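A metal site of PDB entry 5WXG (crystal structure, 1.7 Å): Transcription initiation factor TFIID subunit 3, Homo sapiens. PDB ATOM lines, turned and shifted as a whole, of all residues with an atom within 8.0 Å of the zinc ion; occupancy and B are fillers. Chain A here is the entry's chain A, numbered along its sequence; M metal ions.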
ATOM      1  N   ILE A  15     -34.755 -14.584  -9.259  1.00  0.00           N
ATOM      2  CA  ILE A  15     -33.924 -13.384  -9.365  1.00  0.00           C
ATOM      3  C   ILE A  15     -32.467 -13.820  -9.427  1.00  0.00           C
ATOM      4  O   ILE A  15     -32.052 -14.676  -8.647  1.00  0.00           O
ATOM      5  CB  ILE A  15     -34.145 -12.421  -8.178  1.00  0.00           C
ATOM      6  CG1 ILE A  15     -35.636 -12.118  -7.957  1.00  0.00           C
ATOM      7  CG2 ILE A  15     -33.357 -11.129  -8.364  1.00  0.00           C
ATOM      8  CD1 ILE A  15     -36.343 -11.619  -9.166  1.00  0.00           C
ATOM      9  N   CYS A  16     -31.716 -13.230 -10.329  1.00  0.00           N
ATOM     10  CA  CYS A  16     -30.285 -13.518 -10.469  1.00  0.00           C
ATOM     11  C   CYS A  16     -29.486 -12.859  -9.341  1.00  0.00           C
ATOM     12  O   CYS A  16     -29.513 -11.627  -9.234  1.00  0.00           O
ATOM     13  CB  CYS A  16     -29.799 -13.020 -11.829  1.00  0.00           C
ATOM     14  SG  CYS A  16     -28.027 -13.174 -12.142  1.00  0.00           S
ATOM     15  N   PRO A  17     -28.793 -13.609  -8.486  1.00  0.00           N
ATOM     16  CA  PRO A  17     -27.998 -12.947  -7.438  1.00  0.00           C
ATOM     17  C   PRO A  17     -26.829 -12.164  -7.984  1.00  0.00           C
ATOM     18  O   PRO A  17     -26.281 -11.325  -7.255  1.00  0.00           O
ATOM     19  CB  PRO A  17     -27.542 -14.106  -6.551  1.00  0.00           C
ATOM     20  CG  PRO A  17     -28.499 -15.272  -6.917  1.00  0.00           C
ATOM     21  CD  PRO A  17     -28.747 -15.076  -8.374  1.00  0.00           C
ATOM     22  N   GLY A  18     -26.413 -12.403  -9.234  1.00  0.00           N
ATOM     23  CA  GLY A  18     -25.256 -11.707  -9.779  1.00  0.00           C
ATOM     24  C   GLY A  18     -25.551 -10.263 -10.144  1.00  0.00           C
ATOM     25  O   GLY A  18     -24.751  -9.375  -9.853  1.00  0.00           O
ATOM     26  N   CYS A  19     -26.693 -10.020 -10.793  1.00  0.00           N
ATOM     27  CA  CYS A  19     -27.098  -8.662 -11.142  1.00  0.00           C
ATOM     28  C   CYS A  19     -28.258  -8.159 -10.306  1.00  0.00           C
ATOM     29  O   CYS A  19     -28.587  -6.969 -10.416  1.00  0.00           O
ATOM     30  CB  CYS A  19     -27.453  -8.593 -12.633  1.00  0.00           C
ATOM     31  SG  CYS A  19     -28.941  -9.519 -13.101  1.00  0.00           S
ATOM     32  N   ASN A  20     -28.893  -9.013  -9.503  1.00  0.00           N
ATOM     33  CA  ASN A  20     -30.033  -8.711  -8.639  1.00  0.00           C
ATOM     34  C   ASN A  20     -31.293  -8.346  -9.415  1.00  0.00           C
ATOM     35  O   ASN A  20     -32.222  -7.737  -8.848  1.00  0.00           O
ATOM     36  CB  ASN A  20     -29.675  -7.617  -7.617  1.00  0.00           C
ATOM     37  CG  ASN A  20     -28.768  -8.154  -6.527  1.00  0.00           C
ATOM     38  OD1 ASN A  20     -29.121  -9.113  -5.840  1.00  0.00           O
ATOM     39  ND2 ASN A  20     -27.573  -7.567  -6.390  1.00  0.00           N
ATOM     40  N   LYS A  21     -31.383  -8.769 -10.677  1.00  0.00           N
ATOM     41  CA  LYS A  21     -32.540  -8.527 -11.524  1.00  0.00           C
ATOM     42  C   LYS A  21     -33.239  -9.831 -11.904  1.00  0.00           C
ATOM     43  O   LYS A  21     -32.624 -10.904 -11.915  1.00  0.00           O
ATOM     44  CB  LYS A  21     -32.140  -7.769 -12.795  1.00  0.00           C
ATOM     45  CG  LYS A  21     -31.462  -6.459 -12.511  1.00  0.00           C
ATOM     46  CD  LYS A  21     -31.051  -5.788 -13.789  1.00  0.00           C
ATOM     47  CE  LYS A  21     -30.196  -4.590 -13.477  1.00  0.00           C
ATOM     48  NZ  LYS A  21     -29.542  -4.076 -14.708  1.00  0.00           N
ATOM     49  N   PRO A  22     -34.527  -9.767 -12.232  1.00  0.00           N
ATOM     50  CA  PRO A  22     -35.316 -10.980 -12.484  1.00  0.00           C
ATOM     51  C   PRO A  22     -34.919 -11.710 -13.757  1.00  0.00           C
ATOM     52  O   PRO A  22     -34.298 -11.168 -14.669  1.00  0.00           O
ATOM     53  CB  PRO A  22     -36.753 -10.463 -12.619  1.00  0.00           C
ATOM     54  CG  PRO A  22     -36.755  -9.135 -11.978  1.00  0.00           C
ATOM     55  CD  PRO A  22     -35.374  -8.566 -12.125  1.00  0.00           C
ATOM     56  N   ASP A  23     -35.309 -12.981 -13.790  1.00  0.00           N
ATOM     57  CA  ASP A  23     -35.479 -13.736 -15.031  1.00  0.00           C
ATOM     58  C   ASP A  23     -36.194 -12.867 -16.058  1.00  0.00           C
ATOM     59  O   ASP A  23     -37.304 -12.396 -15.817  1.00  0.00           O
ATOM     60  CB  ASP A  23     -36.287 -15.001 -14.716  1.00  0.00           C
ATOM     61  CG  ASP A  23     -36.724 -15.792 -15.937  1.00  0.00           C
ATOM     62  OD1 ASP A  23     -36.360 -15.455 -17.076  1.00  0.00           O
ATOM     63  OD2 ASP A  23     -37.431 -16.792 -15.726  1.00  0.00           O
ATOM     64  N   ASP A  24     -35.546 -12.626 -17.194  1.00  0.00           N
ATOM     65  CA  ASP A  24     -36.139 -11.837 -18.262  1.00  0.00           C
ATOM     66  C   ASP A  24     -36.321 -12.664 -19.530  1.00  0.00           C
ATOM     67  O   ASP A  24     -36.413 -12.100 -20.626  1.00  0.00           O
ATOM     68  CB  ASP A  24     -35.292 -10.598 -18.562  1.00  0.00           C
ATOM     69  CG  ASP A  24     -33.869 -10.924 -18.973  1.00  0.00           C
ATOM     70  OD1 ASP A  24     -33.538 -12.119 -19.171  1.00  0.00           O
ATOM     71  OD2 ASP A  24     -33.058  -9.981 -19.112  1.00  0.00           O
ATOM     72  N   SER A  26     -34.107 -14.803 -20.784  1.00  0.00           N
ATOM     73  CA  SER A  26     -32.822 -15.170 -21.366  1.00  0.00           C
ATOM     74  C   SER A  26     -32.268 -16.406 -20.646  1.00  0.00           C
ATOM     75  O   SER A  26     -32.793 -16.813 -19.614  1.00  0.00           O
ATOM     76  CB  SER A  26     -31.873 -13.982 -21.287  1.00  0.00           C
ATOM     77  OG  SER A  26     -31.679 -13.540 -19.965  1.00  0.00           O
ATOM     78  N   PRO A  27     -31.216 -17.022 -21.186  1.00  0.00           N
ATOM     79  CA  PRO A  27     -30.739 -18.296 -20.619  1.00  0.00           C
ATOM     80  C   PRO A  27     -30.274 -18.153 -19.180  1.00  0.00           C
ATOM     81  O   PRO A  27     -29.683 -17.136 -18.801  1.00  0.00           O
ATOM     82  CB  PRO A  27     -29.570 -18.675 -21.531  1.00  0.00           C
ATOM     83  CG  PRO A  27     -29.873 -18.008 -22.824  1.00  0.00           C
ATOM     84  CD  PRO A  27     -30.548 -16.712 -22.462  1.00  0.00           C
ATOM     85  N   MET A  28     -30.526 -19.181 -18.376  1.00  0.00           N
ATOM     86  CA  MET A  28     -30.124 -19.171 -16.979  1.00  0.00           C
ATOM     87  C   MET A  28     -29.530 -20.522 -16.630  1.00  0.00           C
ATOM     88  O   MET A  28     -29.729 -21.517 -17.338  1.00  0.00           O
ATOM     89  CB  MET A  28     -31.279 -18.825 -16.038  1.00  0.00           C
ATOM     90  CG  MET A  28     -31.866 -17.434 -16.280  1.00  0.00           C
ATOM     91  SD  MET A  28     -33.148 -16.967 -15.098  1.00  0.00           S
ATOM     92  CE  MET A  28     -32.122 -16.393 -13.737  1.00  0.00           C
ATOM     93  N   TRP A  37     -30.471 -19.378  -9.204  1.00  0.00           N
ATOM     94  CA  TRP A  37     -30.387 -19.353 -10.660  1.00  0.00           C
ATOM     95  C   TRP A  37     -29.857 -18.004 -11.138  1.00  0.00           C
ATOM     96  O   TRP A  37     -30.255 -16.958 -10.639  1.00  0.00           O
ATOM     97  CB  TRP A  37     -31.755 -19.670 -11.299  1.00  0.00           C
ATOM     98  CG  TRP A  37     -32.055 -21.141 -11.229  1.00  0.00           C
ATOM     99  CD1 TRP A  37     -32.450 -21.849 -10.132  1.00  0.00           C
ATOM    100  CD2 TRP A  37     -31.931 -22.085 -12.301  1.00  0.00           C
ATOM    101  NE1 TRP A  37     -32.598 -23.180 -10.458  1.00  0.00           N
ATOM    102  CE2 TRP A  37     -32.291 -23.350 -11.784  1.00  0.00           C
ATOM    103  CE3 TRP A  37     -31.564 -21.987 -13.642  1.00  0.00           C
ATOM    104  CZ2 TRP A  37     -32.273 -24.511 -12.558  1.00  0.00           C
ATOM    105  CZ3 TRP A  37     -31.559 -23.148 -14.420  1.00  0.00           C
ATOM    106  CH2 TRP A  37     -31.910 -24.382 -13.872  1.00  0.00           C
ATOM    107  N   TYR A  38     -28.967 -18.047 -12.124  1.00  0.00           N
ATOM    108  CA  TYR A  38     -28.232 -16.887 -12.622  1.00  0.00           C
ATOM    109  C   TYR A  38     -28.419 -16.738 -14.134  1.00  0.00           C
ATOM    110  O   TYR A  38     -28.443 -17.743 -14.847  1.00  0.00           O
ATOM    111  CB  TYR A  38     -26.720 -17.027 -12.345  1.00  0.00           C
ATOM    112  CG  TYR A  38     -26.258 -16.830 -10.914  1.00  0.00           C
ATOM    113  CD1 TYR A  38     -26.523 -17.779  -9.932  1.00  0.00           C
ATOM    114  CD2 TYR A  38     -25.525 -15.698 -10.557  1.00  0.00           C
ATOM    115  CE1 TYR A  38     -26.080 -17.598  -8.616  1.00  0.00           C
ATOM    116  CE2 TYR A  38     -25.063 -15.515  -9.262  1.00  0.00           C
ATOM    117  CZ  TYR A  38     -25.347 -16.461  -8.297  1.00  0.00           C
ATOM    118  OH  TYR A  38     -24.907 -16.262  -6.992  1.00  0.00           O
ATOM    119  N   HIS A  39     -28.485 -15.493 -14.633  1.00  0.00           N
ATOM    120  CA  HIS A  39     -28.323 -15.269 -16.066  1.00  0.00           C
ATOM    121  C   HIS A  39     -26.923 -15.720 -16.500  1.00  0.00           C
ATOM    122  O   HIS A  39     -25.939 -15.441 -15.805  1.00  0.00           O
ATOM    123  CB  HIS A  39     -28.479 -13.793 -16.433  1.00  0.00           C
ATOM    124  CG  HIS A  39     -29.742 -13.148 -15.951  1.00  0.00           C
ATOM    125  ND1 HIS A  39     -29.742 -12.179 -14.974  1.00  0.00           N
ATOM    126  CD2 HIS A  39     -31.033 -13.286 -16.339  1.00  0.00           C
ATOM    127  CE1 HIS A  39     -30.977 -11.753 -14.766  1.00  0.00           C
ATOM    128  NE2 HIS A  39     -31.781 -12.412 -15.580  1.00  0.00           N
ATOM    129  N   TRP A  40     -26.815 -16.375 -17.659  1.00  0.00           N
ATOM    130  CA  TRP A  40     -25.508 -16.793 -18.157  1.00  0.00           C
ATOM    131  C   TRP A  40     -24.463 -15.690 -18.170  1.00  0.00           C
ATOM    132  O   TRP A  40     -23.357 -15.911 -17.649  1.00  0.00           O
ATOM    133  CB  TRP A  40     -25.621 -17.371 -19.580  1.00  0.00           C
ATOM    134  CG  TRP A  40     -26.200 -18.724 -19.669  1.00  0.00           C
ATOM    135  CD1 TRP A  40     -26.822 -19.431 -18.687  1.00  0.00           C
ATOM    136  CD2 TRP A  40     -26.222 -19.549 -20.837  1.00  0.00           C
ATOM    137  NE1 TRP A  40     -27.233 -20.655 -19.179  1.00  0.00           N
ATOM    138  CE2 TRP A  40     -26.867 -20.752 -20.491  1.00  0.00           C
ATOM    139  CE3 TRP A  40     -25.729 -19.388 -22.143  1.00  0.00           C
ATOM    140  CZ2 TRP A  40     -27.049 -21.787 -21.412  1.00  0.00           C
ATOM    141  CZ3 TRP A  40     -25.921 -20.424 -23.053  1.00  0.00           C
ATOM    142  CH2 TRP A  40     -26.572 -21.602 -22.673  1.00  0.00           C
ATOM    143  N   PRO A  41     -24.692 -14.506 -18.767  1.00  0.00           N
ATOM    144  CA  PRO A  41     -23.615 -13.502 -18.780  1.00  0.00           C
ATOM    145  C   PRO A  41     -23.179 -13.060 -17.408  1.00  0.00           C
ATOM    146  O   PRO A  41     -22.018 -12.669 -17.224  1.00  0.00           O
ATOM    147  CB  PRO A  41     -24.228 -12.337 -19.579  1.00  0.00           C
ATOM    148  CG  PRO A  41     -25.715 -12.573 -19.530  1.00  0.00           C
ATOM    149  CD  PRO A  41     -25.851 -14.055 -19.549  1.00  0.00           C
ATOM    150  N   CYS A  42     -24.063 -13.123 -16.407  1.00  0.00           N
ATOM    151  CA  CYS A  42     -23.680 -12.657 -15.082  1.00  0.00           C
ATOM    152  C   CYS A  42     -22.699 -13.598 -14.393  1.00  0.00           C
ATOM    153  O   CYS A  42     -22.117 -13.213 -13.365  1.00  0.00           O
ATOM    154  CB  CYS A  42     -24.915 -12.453 -14.208  1.00  0.00           C
ATOM    155  SG  CYS A  42     -26.101 -11.272 -14.967  1.00  0.00           S
ATOM    156  N   VAL A  43     -22.513 -14.809 -14.921  1.00  0.00           N
ATOM    157  CA  VAL A  43     -21.490 -15.721 -14.443  1.00  0.00           C
ATOM    158  C   VAL A  43     -20.506 -16.077 -15.563  1.00  0.00           C
ATOM    159  O   VAL A  43     -19.890 -17.147 -15.544  1.00  0.00           O
ATOM    160  CB  VAL A  43     -22.096 -16.984 -13.796  1.00  0.00           C
ATOM    161  CG1 VAL A  43     -22.736 -16.632 -12.463  1.00  0.00           C
ATOM    162  CG2 VAL A  43     -23.118 -17.641 -14.735  1.00  0.00           C
HETATM  163 ZN    ZN M   1     -28.048 -11.536 -13.800  1.00  0.00          ZN
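The backbone carbonyl oxygen of Pro 22 lies within hydrogen-bond range of a ring nitrogen (NE2) of His 39 (3.0 Å).
The backbone NH (N) of Lys 21 lies close to the side-chain sulfur (SG) of Cys 19 (3.5 Å).
The side-chain sulfur (SG) of Cys 16 sits close to the backbone NH (N) of Gly 18.
The backbone NH (N) of Cys 16 lies within hydrogen-bond range of the backbone carbonyl oxygen (O) of Lys 21 (3.0 Å).
ND1 of His 39 binds the zinc ion, at 2.2 Å.
The side-chain sulfur (SG) of Cys 42 is bound to the zinc ion (2.3 Å).
The zinc ion is bound by SG of Cys 19, 2.3 Å away.
SG of Cys 16 binds the zinc ion (2.3 Å).
The zinc ion has four donor atoms within binding distance.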
